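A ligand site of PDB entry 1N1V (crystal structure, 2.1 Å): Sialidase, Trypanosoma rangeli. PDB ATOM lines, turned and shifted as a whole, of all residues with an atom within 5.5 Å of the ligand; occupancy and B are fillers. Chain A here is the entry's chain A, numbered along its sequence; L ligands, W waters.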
ATOM      1  N   ARG A  39     -39.520  13.113 -18.407  1.00  0.00           N
ATOM      2  CA  ARG A  39     -38.355  13.092 -17.524  1.00  0.00           C
ATOM      3  C   ARG A  39     -37.698  14.460 -17.382  1.00  0.00           C
ATOM      4  O   ARG A  39     -38.020  15.422 -18.098  1.00  0.00           O
ATOM      5  CB  ARG A  39     -37.289  12.109 -18.061  1.00  0.00           C
ATOM      6  CG  ARG A  39     -37.637  10.608 -17.885  1.00  0.00           C
ATOM      7  CD  ARG A  39     -36.399   9.696 -17.691  1.00  0.00           C
ATOM      8  NE  ARG A  39     -35.607  10.185 -16.555  1.00  0.00           N
ATOM      9  CZ  ARG A  39     -34.303   9.965 -16.370  1.00  0.00           C
ATOM     10  NH1 ARG A  39     -33.706  10.468 -15.291  1.00  0.00           N
ATOM     11  NH2 ARG A  39     -33.600   9.225 -17.225  1.00  0.00           N
ATOM     12  N   ILE A  40     -36.732  14.530 -16.467  1.00  0.00           N
ATOM     13  CA  ILE A  40     -35.905  15.726 -16.293  1.00  0.00           C
ATOM     14  C   ILE A  40     -36.737  16.977 -15.992  1.00  0.00           C
ATOM     15  O   ILE A  40     -36.690  17.971 -16.723  1.00  0.00           O
ATOM     16  CB  ILE A  40     -35.030  15.947 -17.543  1.00  0.00           C
ATOM     17  CG1 ILE A  40     -34.610  14.608 -18.191  1.00  0.00           C
ATOM     18  CG2 ILE A  40     -33.787  16.791 -17.199  1.00  0.00           C
ATOM     19  CD1 ILE A  40     -33.802  13.655 -17.260  1.00  0.00           C
ATOM     20  N   ASP A  55     -38.493  16.919 -20.427  1.00  0.00           N
ATOM     21  CA  ASP A  55     -38.251  16.097 -21.597  1.00  0.00           C
ATOM     22  C   ASP A  55     -39.573  15.406 -21.915  1.00  0.00           C
ATOM     23  O   ASP A  55     -40.156  14.757 -21.030  1.00  0.00           O
ATOM     24  CB  ASP A  55     -37.266  14.955 -21.286  1.00  0.00           C
ATOM     25  CG  ASP A  55     -35.829  15.322 -21.504  1.00  0.00           C
ATOM     26  OD1 ASP A  55     -35.488  16.525 -21.475  1.00  0.00           O
ATOM     27  OD2 ASP A  55     -34.947  14.452 -21.699  1.00  0.00           O
ATOM     28  N   ARG A  57     -40.275  12.447 -23.872  1.00  0.00           N
ATOM     29  CA  ARG A  57     -39.623  11.330 -24.569  1.00  0.00           C
ATOM     30  C   ARG A  57     -40.756  10.533 -25.224  1.00  0.00           C
ATOM     31  O   ARG A  57     -41.387   9.662 -24.616  1.00  0.00           O
ATOM     32  CB  ARG A  57     -38.758  10.499 -23.590  1.00  0.00           C
ATOM     33  CG  ARG A  57     -37.774  11.381 -22.785  1.00  0.00           C
ATOM     34  CD  ARG A  57     -36.657  10.661 -22.031  1.00  0.00           C
ATOM     35  NE  ARG A  57     -35.616  11.589 -21.588  1.00  0.00           N
ATOM     36  CZ  ARG A  57     -34.419  11.216 -21.176  1.00  0.00           C
ATOM     37  NH1 ARG A  57     -34.112   9.914 -21.113  1.00  0.00           N
ATOM     38  NH2 ARG A  57     -33.527  12.137 -20.814  1.00  0.00           N
ATOM     39  N   ASP A  63     -32.299   7.558 -23.180  1.00  0.00           N
ATOM     40  CA  ASP A  63     -31.642   8.821 -23.442  1.00  0.00           C
ATOM     41  C   ASP A  63     -31.486   9.091 -24.943  1.00  0.00           C
ATOM     42  O   ASP A  63     -31.680  10.214 -25.406  1.00  0.00           O
ATOM     43  CB  ASP A  63     -30.263   8.880 -22.799  1.00  0.00           C
ATOM     44  CG  ASP A  63     -30.309   8.912 -21.275  1.00  0.00           C
ATOM     45  OD1 ASP A  63     -29.242   8.629 -20.678  1.00  0.00           O
ATOM     46  OD2 ASP A  63     -31.325   9.200 -20.587  1.00  0.00           O
ATOM     47  N   MET A  99     -32.762  17.964 -25.111  1.00  0.00           N
ATOM     48  CA  MET A  99     -32.883  17.357 -23.791  1.00  0.00           C
ATOM     49  C   MET A  99     -32.101  18.007 -22.636  1.00  0.00           C
ATOM     50  O   MET A  99     -31.194  18.819 -22.843  1.00  0.00           O
ATOM     51  CB  MET A  99     -32.408  15.888 -23.903  1.00  0.00           C
ATOM     52  CG  MET A  99     -30.895  15.724 -24.228  1.00  0.00           C
ATOM     53  SD  MET A  99     -30.472  14.009 -24.816  1.00  0.00           S
ATOM     54  CE  MET A  99     -31.069  12.980 -23.320  1.00  0.00           C
ATOM     55  N   ASP A 100     -32.467  17.599 -21.417  1.00  0.00           N
ATOM     56  CA  ASP A 100     -31.748  17.987 -20.197  1.00  0.00           C
ATOM     57  C   ASP A 100     -31.760  19.494 -19.992  1.00  0.00           C
ATOM     58  O   ASP A 100     -30.710  20.142 -19.895  1.00  0.00           O
ATOM     59  CB  ASP A 100     -30.299  17.513 -20.270  1.00  0.00           C
ATOM     60  CG  ASP A 100     -30.124  15.999 -19.989  1.00  0.00           C
ATOM     61  OD1 ASP A 100     -31.119  15.231 -19.892  1.00  0.00           O
ATOM     62  OD2 ASP A 100     -28.989  15.507 -19.822  1.00  0.00           O
ATOM     63  N   PHE A 117     -29.191  16.883 -30.258  1.00  0.00           N
ATOM     64  CA  PHE A 117     -28.509  15.811 -30.955  1.00  0.00           C
ATOM     65  C   PHE A 117     -29.323  15.385 -32.174  1.00  0.00           C
ATOM     66  O   PHE A 117     -30.554  15.415 -32.164  1.00  0.00           O
ATOM     67  CB  PHE A 117     -28.280  14.599 -30.029  1.00  0.00           C
ATOM     68  CG  PHE A 117     -27.465  14.924 -28.802  1.00  0.00           C
ATOM     69  CD1 PHE A 117     -28.065  15.507 -27.676  1.00  0.00           C
ATOM     70  CD2 PHE A 117     -26.082  14.677 -28.774  1.00  0.00           C
ATOM     71  CE1 PHE A 117     -27.307  15.822 -26.549  1.00  0.00           C
ATOM     72  CE2 PHE A 117     -25.324  14.992 -27.648  1.00  0.00           C
ATOM     73  CZ  PHE A 117     -25.940  15.559 -26.521  1.00  0.00           C
ATOM     74  N   SER A 123     -24.113   7.305 -25.795  1.00  0.00           N
ATOM     75  CA  SER A 123     -24.028   8.363 -24.804  1.00  0.00           C
ATOM     76  C   SER A 123     -23.037   9.474 -25.149  1.00  0.00           C
ATOM     77  O   SER A 123     -21.881   9.211 -25.577  1.00  0.00           O
ATOM     78  CB  SER A 123     -23.701   7.756 -23.449  1.00  0.00           C
ATOM     79  OG  SER A 123     -24.065   8.618 -22.384  1.00  0.00           O
ATOM     80  N   TRP A 124     -23.489  10.713 -24.922  1.00  0.00           N
ATOM     81  CA  TRP A 124     -22.727  11.913 -25.240  1.00  0.00           C
ATOM     82  C   TRP A 124     -21.277  11.946 -24.769  1.00  0.00           C
ATOM     83  O   TRP A 124     -20.428  12.428 -25.490  1.00  0.00           O
ATOM     84  CB  TRP A 124     -23.469  13.178 -24.763  1.00  0.00           C
ATOM     85  CG  TRP A 124     -23.370  13.434 -23.277  1.00  0.00           C
ATOM     86  CD1 TRP A 124     -23.929  12.711 -22.266  1.00  0.00           C
ATOM     87  CD2 TRP A 124     -22.682  14.517 -22.658  1.00  0.00           C
ATOM     88  NE1 TRP A 124     -23.628  13.278 -21.049  1.00  0.00           N
ATOM     89  CE2 TRP A 124     -22.868  14.397 -21.265  1.00  0.00           C
ATOM     90  CE3 TRP A 124     -21.938  15.602 -23.140  1.00  0.00           C
ATOM     91  CZ2 TRP A 124     -22.325  15.296 -20.362  1.00  0.00           C
ATOM     92  CZ3 TRP A 124     -21.389  16.489 -22.246  1.00  0.00           C
ATOM     93  CH2 TRP A 124     -21.584  16.333 -20.876  1.00  0.00           C
ATOM     94  N   THR A 125     -20.964  11.452 -23.577  1.00  0.00           N
ATOM     95  CA  THR A 125     -19.551  11.518 -23.189  1.00  0.00           C
ATOM     96  C   THR A 125     -18.702  10.547 -24.023  1.00  0.00           C
ATOM     97  O   THR A 125     -17.487  10.662 -24.077  1.00  0.00           O
ATOM     98  CB  THR A 125     -19.315  11.245 -21.697  1.00  0.00           C
ATOM     99  OG1 THR A 125     -19.748   9.902 -21.395  1.00  0.00           O
ATOM    100  CG2 THR A 125     -20.210  12.157 -20.817  1.00  0.00           C
ATOM    101  N   GLN A 199     -21.716  21.043 -17.561  1.00  0.00           N
ATOM    102  CA  GLN A 199     -20.887  19.856 -17.477  1.00  0.00           C
ATOM    103  C   GLN A 199     -20.202  19.688 -18.828  1.00  0.00           C
ATOM    104  O   GLN A 199     -20.846  19.798 -19.865  1.00  0.00           O
ATOM    105  CB  GLN A 199     -21.710  18.610 -17.118  1.00  0.00           C
ATOM    106  CG  GLN A 199     -22.926  18.444 -17.964  1.00  0.00           C
ATOM    107  CD  GLN A 199     -23.952  17.536 -17.321  1.00  0.00           C
ATOM    108  OE1 GLN A 199     -25.152  17.762 -17.460  1.00  0.00           O
ATOM    109  NE2 GLN A 199     -23.487  16.468 -16.681  1.00  0.00           N
ATOM    110  N   SER A 233     -20.472  15.724 -12.607  1.00  0.00           N
ATOM    111  CA  SER A 233     -21.432  15.975 -13.667  1.00  0.00           C
ATOM    112  C   SER A 233     -22.654  16.626 -13.034  1.00  0.00           C
ATOM    113  O   SER A 233     -22.661  16.918 -11.816  1.00  0.00           O
ATOM    114  CB  SER A 233     -21.807  14.674 -14.368  1.00  0.00           C
ATOM    115  OG  SER A 233     -22.583  13.870 -13.484  1.00  0.00           O
ATOM    116  N   GLU A 234     -23.679  16.856 -13.868  1.00  0.00           N
ATOM    117  CA  GLU A 234     -24.949  17.505 -13.490  1.00  0.00           C
ATOM    118  C   GLU A 234     -24.867  18.450 -12.289  1.00  0.00           C
ATOM    119  O   GLU A 234     -25.481  18.240 -11.241  1.00  0.00           O
ATOM    120  CB  GLU A 234     -26.058  16.452 -13.289  1.00  0.00           C
ATOM    121  CG  GLU A 234     -26.515  15.858 -14.617  1.00  0.00           C
ATOM    122  CD  GLU A 234     -27.531  14.742 -14.479  1.00  0.00           C
ATOM    123  OE1 GLU A 234     -27.781  14.254 -13.347  1.00  0.00           O
ATOM    124  OE2 GLU A 234     -28.100  14.339 -15.529  1.00  0.00           O
ATOM    125  N   ARG A 249     -23.218  16.123  -9.110  1.00  0.00           N
ATOM    126  CA  ARG A 249     -23.456  14.690  -9.232  1.00  0.00           C
ATOM    127  C   ARG A 249     -22.057  14.044  -9.346  1.00  0.00           C
ATOM    128  O   ARG A 249     -21.168  14.590 -10.014  1.00  0.00           O
ATOM    129  CB  ARG A 249     -24.219  14.390 -10.530  1.00  0.00           C
ATOM    130  CG  ARG A 249     -24.472  12.886 -10.752  1.00  0.00           C
ATOM    131  CD  ARG A 249     -25.541  12.547 -11.807  1.00  0.00           C
ATOM    132  NE  ARG A 249     -25.440  11.154 -12.292  1.00  0.00           N
ATOM    133  CZ  ARG A 249     -26.281  10.606 -13.154  1.00  0.00           C
ATOM    134  NH1 ARG A 249     -27.290  11.305 -13.647  1.00  0.00           N
ATOM    135  NH2 ARG A 249     -26.110   9.347 -13.558  1.00  0.00           N
ATOM    136  N   ASP A 251     -20.997  10.053  -9.942  1.00  0.00           N
ATOM    137  CA  ASP A 251     -21.260   8.618 -10.078  1.00  0.00           C
ATOM    138  C   ASP A 251     -20.151   7.824  -9.375  1.00  0.00           C
ATOM    139  O   ASP A 251     -18.971   8.072  -9.599  1.00  0.00           O
ATOM    140  CB  ASP A 251     -21.332   8.185 -11.553  1.00  0.00           C
ATOM    141  CG  ASP A 251     -22.502   8.813 -12.291  1.00  0.00           C
ATOM    142  OD1 ASP A 251     -22.296   9.262 -13.441  1.00  0.00           O
ATOM    143  OD2 ASP A 251     -23.650   8.928 -11.802  1.00  0.00           O
ATOM    144  N   GLN A 287     -24.399   4.507  -9.392  1.00  0.00           N
ATOM    145  CA  GLN A 287     -24.734   5.586 -10.303  1.00  0.00           C
ATOM    146  C   GLN A 287     -25.386   6.646  -9.454  1.00  0.00           C
ATOM    147  O   GLN A 287     -26.225   6.317  -8.602  1.00  0.00           O
ATOM    148  CB  GLN A 287     -25.800   5.006 -11.222  1.00  0.00           C
ATOM    149  CG  GLN A 287     -26.252   5.806 -12.409  1.00  0.00           C
ATOM    150  CD  GLN A 287     -27.223   4.942 -13.239  1.00  0.00           C
ATOM    151  OE1 GLN A 287     -27.323   3.713 -13.028  1.00  0.00           O
ATOM    152  NE2 GLN A 287     -27.937   5.577 -14.166  1.00  0.00           N
ATOM    153  N   ASP A 288     -24.995   7.897  -9.654  1.00  0.00           N
ATOM    154  CA  ASP A 288     -25.589   8.985  -8.885  1.00  0.00           C
ATOM    155  C   ASP A 288     -26.834   9.511  -9.609  1.00  0.00           C
ATOM    156  O   ASP A 288     -27.281   8.916 -10.600  1.00  0.00           O
ATOM    157  CB  ASP A 288     -24.568  10.101  -8.631  1.00  0.00           C
ATOM    158  CG  ASP A 288     -24.998  11.043  -7.498  1.00  0.00           C
ATOM    159  OD1 ASP A 288     -26.029  10.769  -6.832  1.00  0.00           O
ATOM    160  OD2 ASP A 288     -24.371  12.082  -7.237  1.00  0.00           O
ATOM    161  N   ARG A 318     -33.504   4.730  -7.753  1.00  0.00           N
ATOM    162  CA  ARG A 318     -33.666   6.074  -7.195  1.00  0.00           C
ATOM    163  C   ARG A 318     -34.897   6.231  -6.320  1.00  0.00           C
ATOM    164  O   ARG A 318     -35.642   7.202  -6.449  1.00  0.00           O
ATOM    165  CB  ARG A 318     -33.624   7.112  -8.322  1.00  0.00           C
ATOM    166  CG  ARG A 318     -32.227   7.314  -8.883  1.00  0.00           C
ATOM    167  CD  ARG A 318     -32.211   7.811 -10.356  1.00  0.00           C
ATOM    168  NE  ARG A 318     -30.847   7.935 -10.879  1.00  0.00           N
ATOM    169  CZ  ARG A 318     -30.567   8.281 -12.141  1.00  0.00           C
ATOM    170  NH1 ARG A 318     -31.560   8.523 -12.991  1.00  0.00           N
ATOM    171  NH2 ARG A 318     -29.311   8.384 -12.552  1.00  0.00           N
ATOM    172  N   TYR A 346     -35.143  12.175 -10.843  1.00  0.00           N
ATOM    173  CA  TYR A 346     -34.801  13.591 -10.954  1.00  0.00           C
ATOM    174  C   TYR A 346     -35.890  14.456 -10.321  1.00  0.00           C
ATOM    175  O   TYR A 346     -37.066  14.081 -10.342  1.00  0.00           O
ATOM    176  CB  TYR A 346     -34.611  14.004 -12.414  1.00  0.00           C
ATOM    177  CG  TYR A 346     -33.294  13.599 -13.052  1.00  0.00           C
ATOM    178  CD1 TYR A 346     -32.656  12.390 -12.718  1.00  0.00           C
ATOM    179  CD2 TYR A 346     -32.679  14.427 -13.984  1.00  0.00           C
ATOM    180  CE1 TYR A 346     -31.418  12.032 -13.333  1.00  0.00           C
ATOM    181  CE2 TYR A 346     -31.470  14.072 -14.591  1.00  0.00           C
ATOM    182  CZ  TYR A 346     -30.859  12.870 -14.282  1.00  0.00           C
ATOM    183  OH  TYR A 346     -29.669  12.565 -14.903  1.00  0.00           O
HETATM  184  C1  LIG L   1     -29.893   9.743 -15.899  1.00  0.00           C
HETATM  185  C2  LIG L   1     -29.518  10.558 -16.950  1.00  0.00           C
HETATM  186  C3  LIG L   1     -30.578  11.454 -17.532  1.00  0.00           C
HETATM  187  C4  LIG L   1     -30.046  12.402 -18.617  1.00  0.00           C
HETATM  188  C5  LIG L   1     -28.798  11.819 -19.260  1.00  0.00           C
HETATM  189  C6  LIG L   1     -27.792  11.532 -18.147  1.00  0.00           C
HETATM  190  C7  LIG L   1     -26.394  11.138 -18.670  1.00  0.00           C
HETATM  191  C8  LIG L   1     -25.472  10.588 -17.584  1.00  0.00           C
HETATM  192  C9  LIG L   1     -24.183  10.066 -18.219  1.00  0.00           C
HETATM  193  C10 LIG L   1     -27.639  12.535 -21.302  1.00  0.00           C
HETATM  194  C11 LIG L   1     -27.324  13.711 -22.159  1.00  0.00           C
HETATM  195  N1  LIG L   1     -28.293  12.806 -20.181  1.00  0.00           N
HETATM  196  O1  LIG L   1     -31.233   9.337 -15.691  1.00  0.00           O
HETATM  197  O2  LIG L   1     -28.979   9.332 -15.082  1.00  0.00           O
HETATM  198  O3  LIG L   1     -31.024  12.573 -19.606  1.00  0.00           O
HETATM  199  O4  LIG L   1     -28.322  10.488 -17.338  1.00  0.00           O
HETATM  200  O5  LIG L   1     -26.486  10.107 -19.649  1.00  0.00           O
HETATM  201  O6  LIG L   1     -25.141  11.601 -16.674  1.00  0.00           O
HETATM  202  O7  LIG L   1     -23.345  11.160 -18.547  1.00  0.00           O
HETATM  203  O8  LIG L   1     -27.256  11.221 -21.646  1.00  0.00           O
HETATM  204  O   HOH W   1     -26.604  11.079 -23.994  1.00  0.00           O
HETATM  205  O   HOH W   2     -28.448   7.897 -18.315  1.00  0.00           O
HETATM  206  O   HOH W   3     -31.100   6.688 -15.921  1.00  0.00           O
HETATM  207  O   HOH W   4     -24.690  13.889 -17.901  1.00  0.00           O
HETATM  208  O   HOH W   5     -23.389  11.492 -14.667  1.00  0.00           O
HETATM  209  O   HOH W   6     -25.230   7.076 -20.296  1.00  0.00           O
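O3 of the ligand sits at hydrogen-bond distance from OD1 of Asp 100, 2.7 Å away. NH2 of Arg 318 is in salt-bridge range of O2 of the ligand (2.7 Å). An oxygen (O1) of the ligand is in salt-bridge range of the guanidinium group (NH1) of Arg 39 (2.7 Å). O3 of the ligand is in hydrogen-bond range of NH2 of Arg 57 (2.8 Å). O2 of the ligand sits close to OH of Tyr 346. The guanidinium group (NH1) of Arg 249 is in salt-bridge range of an oxygen (O2) of the ligand, 3.0 Å away. The indole nitrogen (NE1) of Trp 124 lies within hydrogen-bond range of an oxygen (O7) of the ligand (3.3 Å). An oxygen (O5) of the ligand is in hydrogen-bond range of the side-chain carboxylate (OD1) of Asp 63, 3.3 Å away.
The guanidinium group (NH2) of Arg 318 lies within hydrogen-bond range of the backbone carbonyl oxygen (O) of Asp 288. N of Asp 55 is in hydrogen-bond range of O of Arg 39, 2.8 Å away. The side-chain carboxylate (OD2) of Asp 63 lies within salt-bridge range of the guanidinium group (NH1) of Arg 57, at 2.9 Å. The side-chain carboxylate (OD2) of Asp 55 lies within salt-bridge range of the guanidinium group (NH2) of Arg 57. The side-chain hydroxyl of Tyr 346 lies within hydrogen-bond range of the guanidinium group of Arg 249 (3.0 Å). NH2 of Arg 249 is in hydrogen-bond range of O of Asp 288. OD2 of Asp 251 lies within salt-bridge range of NE of Arg 249, at 2.9 Å. The side-chain amide nitrogen (NE2) of Gln 199 lies close to the backbone NH (N) of Glu 234 (2.8 Å).
Water W1 lies within hydrogen-bond range of an oxygen (O8) of the ligand (2.4 Å) and the backbone NH of Trp 124 (3.3 Å). Water W4 lies within hydrogen-bond range of O6 of the ligand, NE2 of Gln 199 and NE1 of Trp 124. Water W3 lies within hydrogen-bond range of O1 of the ligand and NH1 of Arg 318. Water W5 lies within hydrogen-bond range of O6 of the ligand, OD1 of Asp 251, OG of Ser 233 and NE of Arg 249. Water W2 bridges OD1 of Asp 63 (2.6 Å) and O4 of the ligand (2.8 Å). Water W6 bridges OG of Ser 123 and O5 of the ligand.
CD1 of Ile 40 touches O3 of the ligand (3.8 Å). CE of Met 99 touches O3 of the ligand (3.7 Å). Ser 123 touches the ligand. CG2 of Thr 125 touches O7 of the ligand (3.997 Å). OE2 of Glu 234 touches C6 of the ligand, at 3.9 Å. Hydrophobic or aromatic side chains within 4 Å of the ligand: Ile 40, Met 99, Trp 124 and Tyr 346. Of the 20 residues printed, 13 come within 4 Å of the ligand. The nearest printed residue that does not touch the ligand is Gln 287 (4.003 Å).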
